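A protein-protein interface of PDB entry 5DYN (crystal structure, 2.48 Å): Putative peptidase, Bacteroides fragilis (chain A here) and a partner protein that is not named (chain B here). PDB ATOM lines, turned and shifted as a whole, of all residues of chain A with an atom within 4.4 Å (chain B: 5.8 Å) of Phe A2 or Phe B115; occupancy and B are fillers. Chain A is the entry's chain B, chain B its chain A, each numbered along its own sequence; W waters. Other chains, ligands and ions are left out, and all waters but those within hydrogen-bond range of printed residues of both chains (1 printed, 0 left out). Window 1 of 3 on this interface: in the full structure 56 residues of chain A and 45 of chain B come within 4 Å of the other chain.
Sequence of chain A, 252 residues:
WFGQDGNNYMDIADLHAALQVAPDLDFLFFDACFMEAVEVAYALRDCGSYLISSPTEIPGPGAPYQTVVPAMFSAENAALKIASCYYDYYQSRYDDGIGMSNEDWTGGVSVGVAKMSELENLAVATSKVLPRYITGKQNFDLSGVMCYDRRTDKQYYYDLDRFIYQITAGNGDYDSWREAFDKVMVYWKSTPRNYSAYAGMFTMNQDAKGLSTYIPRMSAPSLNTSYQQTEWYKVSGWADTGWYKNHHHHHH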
ATOM      1  N   TRP A   1      15.383   8.801 -18.133  1.00  0.00           N
ATOM      2  CA  TRP A   1      15.524   7.541 -17.411  1.00  0.00           C
ATOM      3  C   TRP A   1      14.906   7.624 -16.023  1.00  0.00           C
ATOM      4  O   TRP A   1      14.489   8.691 -15.580  1.00  0.00           O
ATOM      5  CB  TRP A   1      17.000   7.145 -17.305  1.00  0.00           C
ATOM      6  CG  TRP A   1      17.891   8.226 -16.751  1.00  0.00           C
ATOM      7  CD1 TRP A   1      18.602   9.146 -17.464  1.00  0.00           C
ATOM      8  CD2 TRP A   1      18.169   8.492 -15.366  1.00  0.00           C
ATOM      9  NE1 TRP A   1      19.303   9.969 -16.615  1.00  0.00           N
ATOM     10  CE2 TRP A   1      19.059   9.586 -15.321  1.00  0.00           C
ATOM     11  CE3 TRP A   1      17.756   7.909 -14.162  1.00  0.00           C
ATOM     12  CZ2 TRP A   1      19.533  10.117 -14.120  1.00  0.00           C
ATOM     13  CZ3 TRP A   1      18.233   8.436 -12.967  1.00  0.00           C
ATOM     14  CH2 TRP A   1      19.112   9.529 -12.958  1.00  0.00           C
ATOM     15  N   PHE A   2      14.836   6.485 -15.345  1.00  0.00           N
ATOM     16  CA  PHE A   2      14.444   6.463 -13.944  1.00  0.00           C
ATOM     17  C   PHE A   2      15.321   5.504 -13.154  1.00  0.00           C
ATOM     18  O   PHE A   2      15.688   4.435 -13.639  1.00  0.00           O
ATOM     19  CB  PHE A   2      12.977   6.068 -13.770  1.00  0.00           C
ATOM     20  CG  PHE A   2      12.647   5.621 -12.374  1.00  0.00           C
ATOM     21  CD1 PHE A   2      12.524   6.548 -11.352  1.00  0.00           C
ATOM     22  CD2 PHE A   2      12.500   4.274 -12.077  1.00  0.00           C
ATOM     23  CE1 PHE A   2      12.247   6.140 -10.060  1.00  0.00           C
ATOM     24  CE2 PHE A   2      12.219   3.862 -10.787  1.00  0.00           C
ATOM     25  CZ  PHE A   2      12.096   4.797  -9.777  1.00  0.00           C
ATOM     26  N   GLY A   3      15.647   5.893 -11.929  1.00  0.00           N
ATOM     27  CA  GLY A   3      16.394   5.033 -11.036  1.00  0.00           C
ATOM     28  C   GLY A   3      17.883   5.054 -11.297  1.00  0.00           C
ATOM     29  O   GLY A   3      18.326   4.954 -12.441  1.00  0.00           O
ATOM     30  N   TYR A   9      21.214   3.072 -14.872  1.00  0.00           N
ATOM     31  CA  TYR A   9      20.003   3.875 -14.953  1.00  0.00           C
ATOM     32  C   TYR A   9      19.016   3.149 -15.857  1.00  0.00           C
ATOM     33  O   TYR A   9      19.381   2.707 -16.943  1.00  0.00           O
ATOM     34  CB  TYR A   9      20.307   5.280 -15.495  1.00  0.00           C
ATOM     35  CG  TYR A   9      21.511   5.951 -14.859  1.00  0.00           C
ATOM     36  CD1 TYR A   9      22.805   5.571 -15.200  1.00  0.00           C
ATOM     37  CD2 TYR A   9      21.354   6.974 -13.930  1.00  0.00           C
ATOM     38  CE1 TYR A   9      23.906   6.168 -14.623  1.00  0.00           C
ATOM     39  CE2 TYR A   9      22.456   7.588 -13.352  1.00  0.00           C
ATOM     40  CZ  TYR A   9      23.729   7.177 -13.705  1.00  0.00           C
ATOM     41  OH  TYR A   9      24.835   7.765 -13.144  1.00  0.00           O
ATOM     42  N   MET A  10      17.775   3.013 -15.413  1.00  0.00           N
ATOM     43  CA  MET A  10      16.790   2.274 -16.188  1.00  0.00           C
ATOM     44  C   MET A  10      16.109   3.151 -17.231  1.00  0.00           C
ATOM     45  O   MET A  10      15.441   4.131 -16.899  1.00  0.00           O
ATOM     46  CB  MET A  10      15.737   1.646 -15.269  1.00  0.00           C
ATOM     47  CG  MET A  10      14.733   0.754 -15.998  1.00  0.00           C
ATOM     48  SD  MET A  10      13.690  -0.213 -14.888  1.00  0.00           S
ATOM     49  CE  MET A  10      13.269   1.039 -13.681  1.00  0.00           C
ATOM     50  N   ILE A  12      13.307   4.207 -19.884  1.00  0.00           N
ATOM     51  CA  ILE A  12      11.856   4.109 -19.767  1.00  0.00           C
ATOM     52  C   ILE A  12      11.309   2.893 -20.514  1.00  0.00           C
ATOM     53  O   ILE A  12      10.369   2.247 -20.051  1.00  0.00           O
ATOM     54  CB  ILE A  12      11.169   5.391 -20.280  1.00  0.00           C
ATOM     55  CG1 ILE A  12      11.618   6.587 -19.446  1.00  0.00           C
ATOM     56  CG2 ILE A  12       9.659   5.263 -20.210  1.00  0.00           C
ATOM     57  CD1 ILE A  12      11.400   6.394 -17.963  1.00  0.00           C
ATOM     58  N   LEU A  15      11.842   0.018 -18.346  1.00  0.00           N
ATOM     59  CA  LEU A  15      10.892   0.106 -17.240  1.00  0.00           C
ATOM     60  C   LEU A  15       9.524  -0.414 -17.671  1.00  0.00           C
ATOM     61  O   LEU A  15       8.896  -1.196 -16.956  1.00  0.00           O
ATOM     62  CB  LEU A  15      10.774   1.546 -16.733  1.00  0.00           C
ATOM     63  CG  LEU A  15       9.653   1.850 -15.733  1.00  0.00           C
ATOM     64  CD1 LEU A  15       9.727   0.939 -14.511  1.00  0.00           C
ATOM     65  CD2 LEU A  15       9.697   3.312 -15.306  1.00  0.00           C
ATOM     66  N   LEU A  19       7.288  -3.611 -16.261  1.00  0.00           N
ATOM     67  CA  LEU A  19       5.960  -3.463 -15.669  1.00  0.00           C
ATOM     68  C   LEU A  19       4.905  -4.332 -16.357  1.00  0.00           C
ATOM     69  O   LEU A  19       3.732  -4.308 -15.980  1.00  0.00           O
ATOM     70  CB  LEU A  19       5.527  -1.996 -15.700  1.00  0.00           C
ATOM     71  CG  LEU A  19       6.275  -1.061 -14.746  1.00  0.00           C
ATOM     72  CD1 LEU A  19       5.827   0.383 -14.924  1.00  0.00           C
ATOM     73  CD2 LEU A  19       6.081  -1.508 -13.305  1.00  0.00           C
ATOM     74  N   LEU A  28       0.634   4.878 -10.751  1.00  0.00           N
ATOM     75  CA  LEU A  28       2.085   4.762 -10.795  1.00  0.00           C
ATOM     76  C   LEU A  28       2.689   6.004 -10.153  1.00  0.00           C
ATOM     77  O   LEU A  28       2.845   7.038 -10.801  1.00  0.00           O
ATOM     78  CB  LEU A  28       2.593   4.594 -12.229  1.00  0.00           C
ATOM     79  CG  LEU A  28       2.523   3.192 -12.844  1.00  0.00           C
ATOM     80  CD1 LEU A  28       1.097   2.827 -13.220  1.00  0.00           C
ATOM     81  CD2 LEU A  28       3.443   3.088 -14.053  1.00  0.00           C
ATOM     82  N   PHE A  29       3.009   5.902  -8.868  1.00  0.00           N
ATOM     83  CA  PHE A  29       3.535   7.038  -8.124  1.00  0.00           C
ATOM     84  C   PHE A  29       5.057   7.087  -8.224  1.00  0.00           C
ATOM     85  O   PHE A  29       5.755   6.237  -7.670  1.00  0.00           O
ATOM     86  CB  PHE A  29       3.091   6.968  -6.657  1.00  0.00           C
ATOM     87  CG  PHE A  29       3.632   8.080  -5.797  1.00  0.00           C
ATOM     88  CD1 PHE A  29       3.892   9.335  -6.331  1.00  0.00           C
ATOM     89  CD2 PHE A  29       3.890   7.865  -4.452  1.00  0.00           C
ATOM     90  CE1 PHE A  29       4.395  10.349  -5.540  1.00  0.00           C
ATOM     91  CE2 PHE A  29       4.392   8.876  -3.657  1.00  0.00           C
ATOM     92  CZ  PHE A  29       4.644  10.121  -4.202  1.00  0.00           C
ATOM     93  N   PHE A  30       5.562   8.089  -8.938  1.00  0.00           N
ATOM     94  CA  PHE A  30       6.998   8.315  -9.042  1.00  0.00           C
ATOM     95  C   PHE A  30       7.465   9.370  -8.047  1.00  0.00           C
ATOM     96  O   PHE A  30       7.442  10.567  -8.338  1.00  0.00           O
ATOM     97  CB  PHE A  30       7.382   8.744 -10.460  1.00  0.00           C
ATOM     98  CG  PHE A  30       7.495   7.605 -11.429  1.00  0.00           C
ATOM     99  CD1 PHE A  30       6.368   7.077 -12.033  1.00  0.00           C
ATOM    100  CD2 PHE A  30       8.731   7.067 -11.742  1.00  0.00           C
ATOM    101  CE1 PHE A  30       6.470   6.030 -12.926  1.00  0.00           C
ATOM    102  CE2 PHE A  30       8.840   6.017 -12.634  1.00  0.00           C
ATOM    103  CZ  PHE A  30       7.707   5.499 -13.227  1.00  0.00           C
ATOM    104  N   ASP A  31       7.885   8.923  -6.869  1.00  0.00           N
ATOM    105  CA  ASP A  31       8.538   9.806  -5.914  1.00  0.00           C
ATOM    106  C   ASP A  31       9.962  10.053  -6.398  1.00  0.00           C
ATOM    107  O   ASP A  31      10.927   9.601  -5.780  1.00  0.00           O
ATOM    108  CB  ASP A  31       8.538   9.200  -4.510  1.00  0.00           C
ATOM    109  CG  ASP A  31       8.615  10.251  -3.421  1.00  0.00           C
ATOM    110  OD1 ASP A  31       8.858  11.434  -3.750  1.00  0.00           O
ATOM    111  OD2 ASP A  31       8.445   9.895  -2.234  1.00  0.00           O
ATOM    112  N   ALA A  32      10.077  10.757  -7.521  1.00  0.00           N
ATOM    113  CA  ALA A  32      11.352  10.964  -8.193  1.00  0.00           C
ATOM    114  C   ALA A  32      11.270  12.187  -9.100  1.00  0.00           C
ATOM    115  O   ALA A  32      10.180  12.627  -9.461  1.00  0.00           O
ATOM    116  CB  ALA A  32      11.740   9.730  -8.991  1.00  0.00           C
ATOM    117  N   MET A  35       9.527  13.190 -13.496  1.00  0.00           N
ATOM    118  CA  MET A  35       8.860  12.035 -14.089  1.00  0.00           C
ATOM    119  C   MET A  35       7.458  12.332 -14.627  1.00  0.00           C
ATOM    120  O   MET A  35       6.875  11.507 -15.335  1.00  0.00           O
ATOM    121  CB  MET A  35       8.787  10.889 -13.078  1.00  0.00           C
ATOM    122  CG  MET A  35      10.147  10.341 -12.673  1.00  0.00           C
ATOM    123  SD  MET A  35      11.276  10.098 -14.062  1.00  0.00           S
ATOM    124  CE  MET A  35      10.434   8.824 -15.003  1.00  0.00           C
ATOM    125  N   LEU B  19       3.340  -2.044  -3.944  1.00  0.00           N
ATOM    126  CA  LEU B  19       4.773  -2.296  -3.888  1.00  0.00           C
ATOM    127  C   LEU B  19       5.541  -0.986  -4.012  1.00  0.00           C
ATOM    128  O   LEU B  19       5.372  -0.251  -4.986  1.00  0.00           O
ATOM    129  CB  LEU B  19       5.196  -3.264  -4.995  1.00  0.00           C
ATOM    130  CG  LEU B  19       6.696  -3.434  -5.254  1.00  0.00           C
ATOM    131  CD1 LEU B  19       7.409  -3.967  -4.024  1.00  0.00           C
ATOM    132  CD2 LEU B  19       6.929  -4.346  -6.446  1.00  0.00           C
ATOM    133  N   VAL B  20       6.374  -0.690  -3.018  1.00  0.00           N
ATOM    134  CA  VAL B  20       7.232   0.487  -3.080  1.00  0.00           C
ATOM    135  C   VAL B  20       8.636   0.069  -3.500  1.00  0.00           C
ATOM    136  O   VAL B  20       9.336  -0.626  -2.763  1.00  0.00           O
ATOM    137  CB  VAL B  20       7.282   1.233  -1.737  1.00  0.00           C
ATOM    138  CG1 VAL B  20       8.215   2.428  -1.830  1.00  0.00           C
ATOM    139  CG2 VAL B  20       5.886   1.684  -1.335  1.00  0.00           C
ATOM    140  N   TYR B  21       9.033   0.484  -4.700  1.00  0.00           N
ATOM    141  CA  TYR B  21      10.302   0.067  -5.283  1.00  0.00           C
ATOM    142  C   TYR B  21      11.371   1.137  -5.081  1.00  0.00           C
ATOM    143  O   TYR B  21      11.352   2.176  -5.738  1.00  0.00           O
ATOM    144  CB  TYR B  21      10.125  -0.235  -6.776  1.00  0.00           C
ATOM    145  CG  TYR B  21      11.209  -1.110  -7.365  1.00  0.00           C
ATOM    146  CD1 TYR B  21      12.433  -0.574  -7.746  1.00  0.00           C
ATOM    147  CD2 TYR B  21      11.008  -2.472  -7.544  1.00  0.00           C
ATOM    148  CE1 TYR B  21      13.427  -1.371  -8.281  1.00  0.00           C
ATOM    149  CE2 TYR B  21      11.997  -3.278  -8.081  1.00  0.00           C
ATOM    150  CZ  TYR B  21      13.203  -2.720  -8.450  1.00  0.00           C
ATOM    151  OH  TYR B  21      14.191  -3.513  -8.988  1.00  0.00           O
ATOM    152  N   ILE B  23      15.033   2.230  -5.494  1.00  0.00           N
ATOM    153  CA  ILE B  23      16.389   2.188  -6.017  1.00  0.00           C
ATOM    154  C   ILE B  23      17.200   3.236  -5.262  1.00  0.00           C
ATOM    155  O   ILE B  23      17.334   4.378  -5.705  1.00  0.00           O
ATOM    156  CB  ILE B  23      16.422   2.449  -7.534  1.00  0.00           C
ATOM    157  CG1 ILE B  23      15.444   1.514  -8.247  1.00  0.00           C
ATOM    158  CG2 ILE B  23      17.835   2.284  -8.076  1.00  0.00           C
ATOM    159  CD1 ILE B  23      15.296   1.788  -9.729  1.00  0.00           C
ATOM    160  N   ALA B  90      18.070  -1.407 -11.045  1.00  0.00           N
ATOM    161  CA  ALA B  90      17.617  -0.621 -12.187  1.00  0.00           C
ATOM    162  C   ALA B  90      17.570  -1.484 -13.442  1.00  0.00           C
ATOM    163  O   ALA B  90      17.364  -0.982 -14.548  1.00  0.00           O
ATOM    164  CB  ALA B  90      18.521   0.582 -12.402  1.00  0.00           C
ATOM    165  N   MET B  95      13.762  -6.102 -11.672  1.00  0.00           N
ATOM    166  CA  MET B  95      12.499  -5.481 -11.290  1.00  0.00           C
ATOM    167  C   MET B  95      11.331  -6.431 -11.542  1.00  0.00           C
ATOM    168  O   MET B  95      10.409  -6.515 -10.733  1.00  0.00           O
ATOM    169  CB  MET B  95      12.290  -4.167 -12.049  1.00  0.00           C
ATOM    170  CG  MET B  95      10.935  -3.527 -11.803  1.00  0.00           C
ATOM    171  SD  MET B  95      10.787  -1.859 -12.471  1.00  0.00           S
ATOM    172  CE  MET B  95      11.606  -0.912 -11.193  1.00  0.00           C
ATOM    173  N   MET B 113       1.801   0.969  -7.447  1.00  0.00           N
ATOM    174  CA  MET B 113       3.245   0.860  -7.313  1.00  0.00           C
ATOM    175  C   MET B 113       3.883   2.229  -7.126  1.00  0.00           C
ATOM    176  O   MET B 113       3.502   3.206  -7.779  1.00  0.00           O
ATOM    177  CB  MET B 113       3.859   0.148  -8.522  1.00  0.00           C
ATOM    178  CG  MET B 113       5.247  -0.417  -8.240  1.00  0.00           C
ATOM    179  SD  MET B 113       5.969  -1.355  -9.599  1.00  0.00           S
ATOM    180  CE  MET B 113       4.622  -2.455  -9.999  1.00  0.00           C
ATOM    181  N   VAL B 114       4.851   2.285  -6.215  1.00  0.00           N
ATOM    182  CA  VAL B 114       5.601   3.500  -5.934  1.00  0.00           C
ATOM    183  C   VAL B 114       7.024   3.365  -6.455  1.00  0.00           C
ATOM    184  O   VAL B 114       7.678   2.339  -6.256  1.00  0.00           O
ATOM    185  CB  VAL B 114       5.631   3.806  -4.424  1.00  0.00           C
ATOM    186  CG1 VAL B 114       6.430   5.071  -4.144  1.00  0.00           C
ATOM    187  CG2 VAL B 114       4.218   3.933  -3.888  1.00  0.00           C
ATOM    188  N   PHE B 115       7.502   4.403  -7.126  1.00  0.00           N
ATOM    189  CA  PHE B 115       8.840   4.383  -7.697  1.00  0.00           C
ATOM    190  C   PHE B 115       9.735   5.398  -6.997  1.00  0.00           C
ATOM    191  O   PHE B 115       9.550   6.609  -7.128  1.00  0.00           O
ATOM    192  CB  PHE B 115       8.768   4.645  -9.199  1.00  0.00           C
ATOM    193  CG  PHE B 115       8.004   3.593  -9.950  1.00  0.00           C
ATOM    194  CD1 PHE B 115       6.625   3.677 -10.082  1.00  0.00           C
ATOM    195  CD2 PHE B 115       8.661   2.508 -10.507  1.00  0.00           C
ATOM    196  CE1 PHE B 115       5.918   2.705 -10.767  1.00  0.00           C
ATOM    197  CE2 PHE B 115       7.958   1.533 -11.195  1.00  0.00           C
ATOM    198  CZ  PHE B 115       6.588   1.633 -11.325  1.00  0.00           C
ATOM    199  N   TRP B 116      10.708   4.876  -6.255  1.00  0.00           N
ATOM    200  CA  TRP B 116      11.509   5.655  -5.316  1.00  0.00           C
ATOM    201  C   TRP B 116      12.977   5.667  -5.727  1.00  0.00           C
ATOM    202  O   TRP B 116      13.694   4.690  -5.486  1.00  0.00           O
ATOM    203  CB  TRP B 116      11.359   5.065  -3.907  1.00  0.00           C
ATOM    204  CG  TRP B 116      11.754   5.963  -2.760  1.00  0.00           C
ATOM    205  CD1 TRP B 116      10.909   6.606  -1.898  1.00  0.00           C
ATOM    206  CD2 TRP B 116      13.086   6.286  -2.330  1.00  0.00           C
ATOM    207  NE1 TRP B 116      11.631   7.314  -0.967  1.00  0.00           N
ATOM    208  CE2 TRP B 116      12.967   7.137  -1.210  1.00  0.00           C
ATOM    209  CE3 TRP B 116      14.365   5.943  -2.783  1.00  0.00           C
ATOM    210  CZ2 TRP B 116      14.078   7.652  -0.543  1.00  0.00           C
ATOM    211  CZ3 TRP B 116      15.465   6.456  -2.120  1.00  0.00           C
ATOM    212  CH2 TRP B 116      15.314   7.301  -1.011  1.00  0.00           C
ATOM    213  N   SER B 117      13.419   6.765  -6.340  1.00  0.00           N
ATOM    214  CA  SER B 117      14.818   6.923  -6.745  1.00  0.00           C
ATOM    215  C   SER B 117      15.085   8.305  -7.337  1.00  0.00           C
ATOM    216  O   SER B 117      14.282   9.223  -7.182  1.00  0.00           O
ATOM    217  CB  SER B 117      15.211   5.853  -7.767  1.00  0.00           C
ATOM    218  OG  SER B 117      16.616   5.760  -7.889  1.00  0.00           O
ATOM    219  N   HIS B 118      16.222   8.444  -8.011  1.00  0.00           N
ATOM    220  CA  HIS B 118      16.486   9.623  -8.831  1.00  0.00           C
ATOM    221  C   HIS B 118      15.692   9.516 -10.125  1.00  0.00           C
ATOM    222  O   HIS B 118      15.374   8.415 -10.574  1.00  0.00           O
ATOM    223  CB  HIS B 118      17.978   9.769  -9.139  1.00  0.00           C
ATOM    224  CG  HIS B 118      18.770  10.370  -8.021  1.00  0.00           C
ATOM    225  ND1 HIS B 118      18.507  11.624  -7.513  1.00  0.00           N
ATOM    226  CD2 HIS B 118      19.828   9.895  -7.321  1.00  0.00           C
ATOM    227  CE1 HIS B 118      19.362  11.892  -6.543  1.00  0.00           C
ATOM    228  NE2 HIS B 118      20.176  10.861  -6.408  1.00  0.00           N
ATOM    229  N   GLY B 119      15.377  10.656 -10.725  1.00  0.00           N
ATOM    230  CA  GLY B 119      14.568  10.676 -11.926  1.00  0.00           C
ATOM    231  C   GLY B 119      15.067  11.669 -12.953  1.00  0.00           C
ATOM    232  O   GLY B 119      15.642  12.702 -12.609  1.00  0.00           O
ATOM    233  N   GLU B 120      14.840  11.349 -14.223  1.00  0.00           N
ATOM    234  CA  GLU B 120      15.279  12.190 -15.327  1.00  0.00           C
ATOM    235  C   GLU B 120      14.395  11.918 -16.544  1.00  0.00           C
ATOM    236  O   GLU B 120      14.888  11.645 -17.638  1.00  0.00           O
ATOM    237  CB  GLU B 120      16.758  11.934 -15.645  1.00  0.00           C
ATOM    238  CG  GLU B 120      17.414  12.923 -16.609  1.00  0.00           C
ATOM    239  CD  GLU B 120      17.564  14.314 -16.025  1.00  0.00           C
ATOM    240  OE1 GLU B 120      18.575  14.565 -15.333  1.00  0.00           O
ATOM    241  OE2 GLU B 120      16.673  15.157 -16.262  1.00  0.00           O
ATOM    242  N   GLY B 121      13.083  11.980 -16.328  1.00  0.00           N
ATOM    243  CA  GLY B 121      12.097  11.850 -17.388  1.00  0.00           C
ATOM    244  C   GLY B 121      12.349  10.735 -18.385  1.00  0.00           C
ATOM    245  O   GLY B 121      12.656   9.605 -18.004  1.00  0.00           O
ATOM    246  N   ILE B 123      14.720  10.854 -20.689  1.00  0.00           N
ATOM    247  CA  ILE B 123      16.135  10.917 -21.069  1.00  0.00           C
ATOM    248  C   ILE B 123      16.830   9.559 -21.026  1.00  0.00           C
ATOM    249  O   ILE B 123      16.689   8.820 -20.056  1.00  0.00           O
ATOM    250  CB  ILE B 123      16.905  11.896 -20.150  1.00  0.00           C
ATOM    251  CG1 ILE B 123      16.327  13.309 -20.263  1.00  0.00           C
ATOM    252  CG2 ILE B 123      18.386  11.908 -20.486  1.00  0.00           C
ATOM    253  CD1 ILE B 123      16.535  13.947 -21.617  1.00  0.00           C
HETATM  254  O   HOH W   1      14.779   6.389 -20.720  1.00  0.00           O
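The backbone NH (N) of Phe A29 is in hydrogen-bond range of the backbone carbonyl oxygen (O) of Met B113. N of Phe B115 lies within hydrogen-bond range of O of Phe A29. O of Phe B115 sits at hydrogen-bond distance from N of Asp A31 (2.9 Å). The backbone carbonyl oxygen (O) of His B118 is in hydrogen-bond range of the backbone NH (N) of Gly A3, 2.9 Å away. O of Glu B120 lies within hydrogen-bond range of N of Trp A1, 2.9 Å away. The backbone NH (N) of Glu B120 lies within hydrogen-bond range of the side-chain sulfur (SD) of Met A35, at 3.8 Å. O of Gly B121 is in hydrogen-bond range of N of Trp A1 (2.8 Å). N of Gly B121 sits at hydrogen-bond distance from SD of Met A35. N of Trp A1 lies close to O of Ile B123, 2.3 Å away. The side-chain sulfur (SD) of Met A10 lies close to the backbone carbonyl oxygen (O) of Ala B90, 3.8 Å away.
The backbone carbonyl oxygen of Leu B19 is in hydrogen-bond range of the backbone NH of Val B114 (2.9 Å). The backbone carbonyl oxygen (O) of Val B114 is in hydrogen-bond range of the backbone NH (N) of Tyr B21 (2.8 Å). N of Trp B116 lies within hydrogen-bond range of O of Tyr B21 (2.8 Å). O of Trp B116 lies within hydrogen-bond range of N of Ile B23 (2.8 Å). The side-chain hydroxyl of Ser B117 lies within hydrogen-bond range of the backbone carbonyl oxygen of Ile B23, 2.7 Å away. The backbone NH of Phe A2 lies within hydrogen-bond range of the backbone carbonyl oxygen of Met A10 (2.9 Å).
His B118 touches Trp A1 (O to CZ3, 3.7 Å). Phe A2 touches Ile B23 (CE2 to CD1, 3.9 Å). Phe A2 touches Phe B115. Gly A3 touches Ser B117 (CA to OG, 3.2 Å). CE of Met A10 touches CE of Met B95, 3.6 Å away. CD2 of Leu A19 touches SD of Met B113, at 3.7 Å. Leu A19 touches Phe B115. CD2 of Phe A30 touches CB of Phe B115, at 3.5 Å. Asp A31 touches Ser B117. Met A35 touches Gly B119.
Printed residues of chain B within 4 Å of Leu A28: Met B113 (3.7 Å). Printed residues of chain B within 4 Å of Phe A29: Met B113, Val B114 and Phe B115. Of the printed residues of chain B, Met A35 touches Gly B119, Glu B120 and Gly B121. Printed residues of chain A within 4 Å of Phe B115: Phe A2, Leu A15, Leu A19, Phe A29, Phe A30 and Asp A31. Of the printed residues of chain A, Ser B117 touches Phe A2, Gly A3, Asp A31 and Ala A32. The nearest printed residue of chain A that does not touch Phe B115 is Leu A28 (4.01 Å). The nearest printed residue of chain B that does not touch Leu A28 is Phe B115 (4.01 Å).
Of the 16 printed residues of chain B, 13 touch a printed residue of chain A. Printed residues of chain B that touch a printed residue of chain A: Ile B23, Ala B90, Met B95, Met B113, Val B114, Phe B115, Trp B116, Ser B117, His B118, Gly B119, Glu B120, Gly B121 and Ile B123. Among the printed residues, 30 pairs touch across the chains.
Water W1 bridges the backbone NH (N) of Ile A12 (2.8 Å) and the backbone carbonyl oxygen (O) of Ile B123 (3.2 Å).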
